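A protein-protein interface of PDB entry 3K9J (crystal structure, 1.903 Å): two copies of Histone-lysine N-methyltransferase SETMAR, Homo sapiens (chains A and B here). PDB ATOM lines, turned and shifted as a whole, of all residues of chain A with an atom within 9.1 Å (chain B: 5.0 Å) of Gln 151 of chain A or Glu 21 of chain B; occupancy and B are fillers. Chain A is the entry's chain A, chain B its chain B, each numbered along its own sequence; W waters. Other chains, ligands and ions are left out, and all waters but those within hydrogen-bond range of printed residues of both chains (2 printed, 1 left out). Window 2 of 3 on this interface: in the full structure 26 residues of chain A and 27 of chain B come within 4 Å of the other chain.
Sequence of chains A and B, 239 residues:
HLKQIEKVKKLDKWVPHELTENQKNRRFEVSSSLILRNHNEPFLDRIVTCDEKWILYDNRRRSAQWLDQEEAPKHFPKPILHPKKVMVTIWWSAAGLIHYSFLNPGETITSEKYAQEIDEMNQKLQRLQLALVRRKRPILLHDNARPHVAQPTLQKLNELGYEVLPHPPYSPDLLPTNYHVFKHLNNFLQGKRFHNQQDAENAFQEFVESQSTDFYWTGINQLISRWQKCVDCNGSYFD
The side-chain amide oxygen of Gln 151 of chain A is in hydrogen-bond range of the side-chain amide nitrogen of Asn 25 of chain B, at 2.6 Å. The side-chain amide oxygen (OD1) of Asn 25 of chain B lies close to the backbone carbonyl oxygen (O) of Val 149 of chain A (3.4 Å). The side-chain amide oxygen (OD1) of Asn 234 of chain B sits at hydrogen-bond distance from the side-chain amide nitrogen (NE2) of Gln 155 of chain A, 2.8 Å away. NH2 of Arg 146 of chain A sits at hydrogen-bond distance from OD1 of Asn 22 of chain B, 2.6 Å away.
The side-chain amide nitrogen of Asn 25 of chain B sits close to the backbone carbonyl oxygen of Glu 21 of chain B (3.4 Å). The side-chain hydroxyl of Thr 20 of chain B lies close to the backbone NH of Asn 22 of chain B, at 3.5 Å. OE1 of Gln 155 of chain A sits close to O of Gln 151 of chain A (3.3 Å).
Asn 25 of chain B touches Ala 150 of chain A (OD1 to CA, 3.7 Å). Glu 21 of chain B touches Gln 151 of chain A (OE2 to OE1, 3.9 Å). CD1 of Phe 28 of chain B touches NE2 of Gln 151 of chain A, 3.3 Å away. Gln 151 of chain A touches Asn 234 of chain B. Asn 25 of chain B touches Leu 154 of chain A (O to CD1, 3.5 Å). CE2 of Phe 28 of chain B touches O of Leu 154 of chain A, at 3.6 Å. Gln 155 of chain A touches Phe 28 of chain B.
Of the printed residues of chain B, Val 149 of chain A touches Asn 25. Printed residues of chain B within 4 Å of Ala 150 of chain A: Asn 25. Gln 151 of chain A touches four residues of chain B. No residue of chain A comes within 4 Å of Thr 20 of chain B. Glu 21 of chain B touches one residue of chain A. The nearest residue of chain B that does not touch Gln 151 of chain A is Lys 24 of chain B (4.7 Å).
Of the 9 printed residues of chain B, 5 touch a printed residue of chain A. Hydrophobic or aromatic side chains of chain B within 4 Å of the printed part of chain A: Phe 28. Of the 18 printed residues of chain A, 6 touch a printed residue of chain B. Printed residues of chain A that touch a printed residue of chain B: Arg 146, Val 149, Ala 150, Gln 151, Leu 154 and Gln 155.
No position is printed for both chains. Of the 11 pairs that touch across the chains among the printed residues, none has its exchanged pair printed and touching as well.
Water W1 lies within hydrogen-bond range of the backbone NH of Gln 151 of chain A (2.8 Å) and the side-chain amide oxygen of Asn 25 of chain B (3.2 Å). Water W2 bridges OD1 of Asn 22 of chain B (3.1 Å) and NE of Arg 146 of chain A (3.2 Å).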
ATOM      1  N   SER A 111     -18.757  26.029  13.072  1.00  0.00           N
ATOM      2  CA  SER A 111     -19.070  24.782  12.381  1.00  0.00           C
ATOM      3  C   SER A 111     -19.065  24.966  10.869  1.00  0.00           C
ATOM      4  O   SER A 111     -18.561  24.117  10.141  1.00  0.00           O
ATOM      5  CB  SER A 111     -20.405  24.194  12.842  1.00  0.00           C
ATOM      6  OG  SER A 111     -20.523  22.858  12.386  1.00  0.00           O
ATOM      7  N   GLU A 112     -19.619  26.082  10.406  1.00  0.00           N
ATOM      8  CA  GLU A 112     -19.610  26.419   8.983  1.00  0.00           C
ATOM      9  C   GLU A 112     -18.187  26.503   8.422  1.00  0.00           C
ATOM     10  O   GLU A 112     -17.948  26.167   7.263  1.00  0.00           O
ATOM     11  CB  GLU A 112     -20.340  27.743   8.736  1.00  0.00           C
ATOM     12  CG  GLU A 112     -21.865  27.644   8.705  1.00  0.00           C
ATOM     13  CD  GLU A 112     -22.502  27.560  10.093  1.00  0.00           C
ATOM     14  OE1 GLU A 112     -23.755  27.588  10.168  1.00  0.00           O
ATOM     15  OE2 GLU A 112     -21.757  27.466  11.100  1.00  0.00           O
ATOM     16  N   ALA A 115     -16.501  22.985   8.409  1.00  0.00           N
ATOM     17  CA  ALA A 115     -16.994  22.318   7.204  1.00  0.00           C
ATOM     18  C   ALA A 115     -16.201  22.768   5.979  1.00  0.00           C
ATOM     19  O   ALA A 115     -15.866  21.968   5.098  1.00  0.00           O
ATOM     20  CB  ALA A 115     -18.476  22.597   7.005  1.00  0.00           C
ATOM     21  N   ILE A 118     -12.723  21.222   6.178  1.00  0.00           N
ATOM     22  CA  ILE A 118     -12.827  19.807   5.855  1.00  0.00           C
ATOM     23  C   ILE A 118     -12.771  19.676   4.343  1.00  0.00           C
ATOM     24  O   ILE A 118     -12.025  18.866   3.795  1.00  0.00           O
ATOM     25  CB  ILE A 118     -14.136  19.193   6.435  1.00  0.00           C
ATOM     26  CG1 ILE A 118     -14.016  19.065   7.956  1.00  0.00           C
ATOM     27  CG2 ILE A 118     -14.419  17.833   5.813  1.00  0.00           C
ATOM     28  CD1 ILE A 118     -15.307  18.658   8.657  1.00  0.00           C
ATOM     29  N   ARG A 146     -17.542  21.463  20.507  1.00  0.00           N
ATOM     30  CA  ARG A 146     -18.901  21.704  20.044  1.00  0.00           C
ATOM     31  C   ARG A 146     -19.026  22.029  18.553  1.00  0.00           C
ATOM     32  O   ARG A 146     -19.919  21.508  17.879  1.00  0.00           O
ATOM     33  CB  ARG A 146     -19.629  22.719  20.928  1.00  0.00           C
ATOM     34  CG  ARG A 146     -19.722  22.266  22.386  1.00  0.00           C
ATOM     35  CD  ARG A 146     -21.032  22.680  23.044  1.00  0.00           C
ATOM     36  NE  ARG A 146     -22.109  21.713  22.825  1.00  0.00           N
ATOM     37  CZ  ARG A 146     -23.241  21.682  23.526  1.00  0.00           C
ATOM     38  NH1 ARG A 146     -23.451  22.561  24.495  1.00  0.00           N
ATOM     39  NH2 ARG A 146     -24.164  20.768  23.265  1.00  0.00           N
ATOM     40  N   PRO A 147     -18.140  22.884  18.023  1.00  0.00           N
ATOM     41  CA  PRO A 147     -18.159  23.082  16.565  1.00  0.00           C
ATOM     42  C   PRO A 147     -17.899  21.775  15.794  1.00  0.00           C
ATOM     43  O   PRO A 147     -18.390  21.629  14.673  1.00  0.00           O
ATOM     44  CB  PRO A 147     -17.008  24.081  16.331  1.00  0.00           C
ATOM     45  CG  PRO A 147     -16.191  24.026  17.610  1.00  0.00           C
ATOM     46  CD  PRO A 147     -17.202  23.806  18.679  1.00  0.00           C
ATOM     47  N   HIS A 148     -17.144  20.850  16.398  1.00  0.00           N
ATOM     48  CA  HIS A 148     -16.822  19.544  15.802  1.00  0.00           C
ATOM     49  C   HIS A 148     -18.043  18.638  15.686  1.00  0.00           C
ATOM     50  O   HIS A 148     -18.085  17.739  14.845  1.00  0.00           O
ATOM     51  CB  HIS A 148     -15.774  18.807  16.647  1.00  0.00           C
ATOM     52  CG  HIS A 148     -14.395  19.396  16.582  1.00  0.00           C
ATOM     53  ND1 HIS A 148     -13.290  18.757  17.108  1.00  0.00           N
ATOM     54  CD2 HIS A 148     -13.937  20.555  16.049  1.00  0.00           C
ATOM     55  CE1 HIS A 148     -12.216  19.502  16.913  1.00  0.00           C
ATOM     56  NE2 HIS A 148     -12.578  20.595  16.270  1.00  0.00           N
ATOM     57  N   VAL A 149     -19.027  18.860  16.545  1.00  0.00           N
ATOM     58  CA  VAL A 149     -20.165  17.957  16.631  1.00  0.00           C
ATOM     59  C   VAL A 149     -21.494  18.533  16.115  1.00  0.00           C
ATOM     60  O   VAL A 149     -22.546  17.940  16.374  1.00  0.00           O
ATOM     61  CB  VAL A 149     -20.356  17.438  18.087  1.00  0.00           C
ATOM     62  CG1 VAL A 149     -19.107  16.683  18.561  1.00  0.00           C
ATOM     63  CG2 VAL A 149     -20.671  18.589  19.031  1.00  0.00           C
ATOM     64  N   ALA A 150     -21.445  19.647  15.371  1.00  0.00           N
ATOM     65  CA  ALA A 150     -22.664  20.339  14.891  1.00  0.00           C
ATOM     66  C   ALA A 150     -23.058  20.094  13.416  1.00  0.00           C
ATOM     67  O   ALA A 150     -22.253  19.644  12.602  1.00  0.00           O
ATOM     68  CB  ALA A 150     -22.566  21.834  15.167  1.00  0.00           C
ATOM     69  N   GLN A 151     -24.298  20.437  13.066  1.00  0.00           N
ATOM     70  CA  GLN A 151     -24.916  19.902  11.839  1.00  0.00           C
ATOM     71  C   GLN A 151     -24.243  20.211  10.492  1.00  0.00           C
ATOM     72  O   GLN A 151     -24.197  19.337   9.624  1.00  0.00           O
ATOM     73  CB  GLN A 151     -26.429  20.180  11.797  1.00  0.00           C
ATOM     74  CG  GLN A 151     -27.251  19.193  10.944  1.00  0.00           C
ATOM     75  CD  GLN A 151     -27.307  17.770  11.498  1.00  0.00           C
ATOM     76  OE1 GLN A 151     -27.843  17.517  12.587  1.00  0.00           O
ATOM     77  NE2 GLN A 151     -26.775  16.823  10.731  1.00  0.00           N
ATOM     78  N   PRO A 152     -23.719  21.439  10.298  1.00  0.00           N
ATOM     79  CA  PRO A 152     -23.077  21.660   8.997  1.00  0.00           C
ATOM     80  C   PRO A 152     -21.829  20.793   8.834  1.00  0.00           C
ATOM     81  O   PRO A 152     -21.561  20.260   7.752  1.00  0.00           O
ATOM     82  CB  PRO A 152     -22.686  23.147   9.033  1.00  0.00           C
ATOM     83  CG  PRO A 152     -23.431  23.734  10.203  1.00  0.00           C
ATOM     84  CD  PRO A 152     -23.629  22.616  11.176  1.00  0.00           C
ATOM     85  N   THR A 153     -21.069  20.653   9.911  1.00  0.00           N
ATOM     86  CA  THR A 153     -19.906  19.781   9.899  1.00  0.00           C
ATOM     87  C   THR A 153     -20.281  18.320   9.635  1.00  0.00           C
ATOM     88  O   THR A 153     -19.673  17.651   8.802  1.00  0.00           O
ATOM     89  CB  THR A 153     -19.127  19.897  11.216  1.00  0.00           C
ATOM     90  OG1 THR A 153     -18.419  21.148  11.231  1.00  0.00           O
ATOM     91  CG2 THR A 153     -18.134  18.753  11.352  1.00  0.00           C
ATOM     92  N   LEU A 154     -21.284  17.831  10.350  1.00  0.00           N
ATOM     93  CA  LEU A 154     -21.718  16.446  10.196  1.00  0.00           C
ATOM     94  C   LEU A 154     -22.221  16.164   8.779  1.00  0.00           C
ATOM     95  O   LEU A 154     -21.923  15.118   8.199  1.00  0.00           O
ATOM     96  CB  LEU A 154     -22.794  16.112  11.233  1.00  0.00           C
ATOM     97  CG  LEU A 154     -22.381  16.272  12.698  1.00  0.00           C
ATOM     98  CD1 LEU A 154     -23.553  15.993  13.611  1.00  0.00           C
ATOM     99  CD2 LEU A 154     -21.182  15.369  13.059  1.00  0.00           C
ATOM    100  N   GLN A 155     -22.973  17.111   8.216  1.00  0.00           N
ATOM    101  CA  GLN A 155     -23.490  16.967   6.860  1.00  0.00           C
ATOM    102  C   GLN A 155     -22.339  16.880   5.859  1.00  0.00           C
ATOM    103  O   GLN A 155     -22.358  16.084   4.912  1.00  0.00           O
ATOM    104  CB  GLN A 155     -24.388  18.159   6.512  1.00  0.00           C
ATOM    105  CG  GLN A 155     -25.779  17.768   6.059  1.00  0.00           C
ATOM    106  CD  GLN A 155     -26.825  18.015   7.133  1.00  0.00           C
ATOM    107  OE1 GLN A 155     -26.910  19.110   7.694  1.00  0.00           O
ATOM    108  NE2 GLN A 155     -27.639  17.003   7.411  1.00  0.00           N
ATOM    109  N   LYS A 156     -21.324  17.697   6.074  1.00  0.00           N
ATOM    110  CA  LYS A 156     -20.154  17.695   5.209  1.00  0.00           C
ATOM    111  C   LYS A 156     -19.391  16.360   5.299  1.00  0.00           C
ATOM    112  O   LYS A 156     -18.983  15.787   4.286  1.00  0.00           O
ATOM    113  CB  LYS A 156     -19.242  18.879   5.568  1.00  0.00           C
ATOM    114  CG  LYS A 156     -17.926  18.922   4.812  1.00  0.00           C
ATOM    115  CD  LYS A 156     -18.116  19.212   3.332  1.00  0.00           C
ATOM    116  CE  LYS A 156     -18.757  20.571   3.113  1.00  0.00           C
ATOM    117  NZ  LYS A 156     -18.944  20.859   1.654  1.00  0.00           N
ATOM    118  N   LEU A 157     -19.214  15.849   6.509  1.00  0.00           N
ATOM    119  CA  LEU A 157     -18.498  14.587   6.665  1.00  0.00           C
ATOM    120  C   LEU A 157     -19.274  13.457   5.978  1.00  0.00           C
ATOM    121  O   LEU A 157     -18.685  12.609   5.305  1.00  0.00           O
ATOM    122  CB  LEU A 157     -18.237  14.284   8.156  1.00  0.00           C
ATOM    123  CG  LEU A 157     -17.218  15.256   8.788  1.00  0.00           C
ATOM    124  CD1 LEU A 157     -17.219  15.118  10.295  1.00  0.00           C
ATOM    125  CD2 LEU A 157     -15.810  15.050   8.231  1.00  0.00           C
ATOM    126  N   ASN A 158     -20.595  13.467   6.130  1.00  0.00           N
ATOM    127  CA  ASN A 158     -21.461  12.475   5.490  1.00  0.00           C
ATOM    128  C   ASN A 158     -21.403  12.579   3.971  1.00  0.00           C
ATOM    129  O   ASN A 158     -21.329  11.573   3.277  1.00  0.00           O
ATOM    130  CB  ASN A 158     -22.913  12.604   5.991  1.00  0.00           C
ATOM    131  CG  ASN A 158     -23.851  11.598   5.335  1.00  0.00           C
ATOM    132  OD1 ASN A 158     -23.734  10.382   5.538  1.00  0.00           O
ATOM    133  ND2 ASN A 158     -24.780  12.099   4.536  1.00  0.00           N
ATOM    134  N   GLU A 159     -21.391  13.809   3.463  1.00  0.00           N
ATOM    135  CA  GLU A 159     -21.320  14.062   2.031  1.00  0.00           C
ATOM    136  C   GLU A 159     -20.000  13.585   1.412  1.00  0.00           C
ATOM    137  O   GLU A 159     -19.984  13.031   0.308  1.00  0.00           O
ATOM    138  CB  GLU A 159     -21.515  15.562   1.783  1.00  0.00           C
ATOM    139  CG  GLU A 159     -21.223  16.029   0.374  1.00  0.00           C
ATOM    140  CD  GLU A 159     -21.005  17.537   0.303  1.00  0.00           C
ATOM    141  OE1 GLU A 159     -21.661  18.275   1.077  1.00  0.00           O
ATOM    142  OE2 GLU A 159     -20.176  17.983  -0.522  1.00  0.00           O
ATOM    143  N   LEU B  19     -36.337  15.705  20.991  1.00  0.00           N
ATOM    144  CA  LEU B  19     -34.894  15.512  21.025  1.00  0.00           C
ATOM    145  C   LEU B  19     -34.199  16.860  20.927  1.00  0.00           C
ATOM    146  O   LEU B  19     -34.551  17.685  20.083  1.00  0.00           O
ATOM    147  CB  LEU B  19     -34.447  14.607  19.874  1.00  0.00           C
ATOM    148  CG  LEU B  19     -34.804  13.124  19.997  1.00  0.00           C
ATOM    149  CD1 LEU B  19     -34.677  12.435  18.643  1.00  0.00           C
ATOM    150  CD2 LEU B  19     -33.920  12.458  21.025  1.00  0.00           C
ATOM    151  N   THR B  20     -33.220  17.086  21.795  1.00  0.00           N
ATOM    152  CA  THR B  20     -32.409  18.286  21.702  1.00  0.00           C
ATOM    153  C   THR B  20     -31.624  18.230  20.402  1.00  0.00           C
ATOM    154  O   THR B  20     -31.491  17.167  19.796  1.00  0.00           O
ATOM    155  CB  THR B  20     -31.435  18.388  22.875  1.00  0.00           C
ATOM    156  OG1 THR B  20     -30.450  17.353  22.770  1.00  0.00           O
ATOM    157  CG2 THR B  20     -32.184  18.235  24.189  1.00  0.00           C
ATOM    158  N   GLU B  21     -31.111  19.376  19.970  1.00  0.00           N
ATOM    159  CA  GLU B  21     -30.321  19.437  18.751  1.00  0.00           C
ATOM    160  C   GLU B  21     -29.082  18.554  18.905  1.00  0.00           C
ATOM    161  O   GLU B  21     -28.624  17.940  17.942  1.00  0.00           O
ATOM    162  CB  GLU B  21     -29.930  20.883  18.431  1.00  0.00           C
ATOM    163  CG  GLU B  21     -29.358  21.098  17.026  1.00  0.00           C
ATOM    164  CD  GLU B  21     -30.306  20.636  15.916  1.00  0.00           C
ATOM    165  OE1 GLU B  21     -31.504  21.006  15.955  1.00  0.00           O
ATOM    166  OE2 GLU B  21     -29.846  19.904  15.002  1.00  0.00           O
ATOM    167  N   ASN B  22     -28.548  18.475  20.117  1.00  0.00           N
ATOM    168  CA  ASN B  22     -27.356  17.670  20.336  1.00  0.00           C
ATOM    169  C   ASN B  22     -27.644  16.176  20.305  1.00  0.00           C
ATOM    170  O   ASN B  22     -26.825  15.386  19.854  1.00  0.00           O
ATOM    171  CB  ASN B  22     -26.646  18.078  21.632  1.00  0.00           C
ATOM    172  CG  ASN B  22     -25.728  19.273  21.433  1.00  0.00           C
ATOM    173  OD1 ASN B  22     -24.521  19.117  21.257  1.00  0.00           O
ATOM    174  ND2 ASN B  22     -26.304  20.470  21.421  1.00  0.00           N
ATOM    175  N   GLN B  23     -28.818  15.794  20.780  1.00  0.00           N
ATOM    176  CA  GLN B  23     -29.230  14.406  20.688  1.00  0.00           C
ATOM    177  C   GLN B  23     -29.465  14.004  19.228  1.00  0.00           C
ATOM    178  O   GLN B  23     -29.190  12.871  18.842  1.00  0.00           O
ATOM    179  CB  GLN B  23     -30.475  14.155  21.548  1.00  0.00           C
ATOM    180  CG  GLN B  23     -30.208  14.215  23.058  1.00  0.00           C
ATOM    181  CD  GLN B  23     -31.484  14.387  23.879  1.00  0.00           C
ATOM    182  OE1 GLN B  23     -32.532  14.765  23.353  1.00  0.00           O
ATOM    183  NE2 GLN B  23     -31.391  14.122  25.176  1.00  0.00           N
ATOM    184  N   LYS B  24     -29.963  14.935  18.415  1.00  0.00           N
ATOM    185  CA  LYS B  24     -30.123  14.700  16.981  1.00  0.00           C
ATOM    186  C   LYS B  24     -28.780  14.637  16.254  1.00  0.00           C
ATOM    187  O   LYS B  24     -28.589  13.820  15.359  1.00  0.00           O
ATOM    188  CB  LYS B  24     -30.995  15.784  16.346  1.00  0.00           C
ATOM    189  CG  LYS B  24     -32.455  15.744  16.783  1.00  0.00           C
ATOM    190  CD  LYS B  24     -33.271  16.789  16.029  1.00  0.00           C
ATOM    191  CE  LYS B  24     -34.768  16.533  16.169  1.00  0.00           C
ATOM    192  NZ  LYS B  24     -35.584  17.339  15.202  1.00  0.00           N
ATOM    193  N   ASN B  25     -27.853  15.517  16.621  1.00  0.00           N
ATOM    194  CA  ASN B  25     -26.522  15.465  16.037  1.00  0.00           C
ATOM    195  C   ASN B  25     -25.838  14.129  16.352  1.00  0.00           C
ATOM    196  O   ASN B  25     -25.129  13.567  15.517  1.00  0.00           O
ATOM    197  CB  ASN B  25     -25.662  16.633  16.539  1.00  0.00           C
ATOM    198  CG  ASN B  25     -26.126  17.991  15.994  1.00  0.00           C
ATOM    199  OD1 ASN B  25     -25.716  19.042  16.498  1.00  0.00           O
ATOM    200  ND2 ASN B  25     -26.975  17.973  14.968  1.00  0.00           N
ATOM    201  N   PHE B  28     -27.414  11.394  14.198  1.00  0.00           N
ATOM    202  CA  PHE B  28     -26.896  11.626  12.850  1.00  0.00           C
ATOM    203  C   PHE B  28     -25.465  11.119  12.660  1.00  0.00           C
ATOM    204  O   PHE B  28     -25.165  10.377  11.712  1.00  0.00           O
ATOM    205  CB  PHE B  28     -26.960  13.121  12.504  1.00  0.00           C
ATOM    206  CG  PHE B  28     -26.623  13.420  11.072  1.00  0.00           C
ATOM    207  CD1 PHE B  28     -27.633  13.669  10.145  1.00  0.00           C
ATOM    208  CD2 PHE B  28     -25.309  13.467  10.646  1.00  0.00           C
ATOM    209  CE1 PHE B  28     -27.330  13.940   8.826  1.00  0.00           C
ATOM    210  CE2 PHE B  28     -25.001  13.737   9.325  1.00  0.00           C
ATOM    211  CZ  PHE B  28     -26.024  13.973   8.412  1.00  0.00           C
ATOM    212  N   ASN B 234     -31.991  14.181   9.407  1.00  0.00           N
ATOM    213  CA  ASN B 234     -31.058  15.024  10.149  1.00  0.00           C
ATOM    214  C   ASN B 234     -30.989  14.639  11.622  1.00  0.00           C
ATOM    215  O   ASN B 234     -30.868  15.502  12.483  1.00  0.00           O
ATOM    216  CB  ASN B 234     -31.418  16.511  10.017  1.00  0.00           C
ATOM    217  CG  ASN B 234     -31.216  17.045   8.608  1.00  0.00           C
ATOM    218  OD1 ASN B 234     -30.331  16.597   7.877  1.00  0.00           O
ATOM    219  ND2 ASN B 234     -32.036  18.018   8.222  1.00  0.00           N
HETATM  220  O   HOH W   1     -26.458  21.425  14.506  1.00  0.00           O
HETATM  221  O   HOH W   2     -22.607  21.070  19.731  1.00  0.00           O
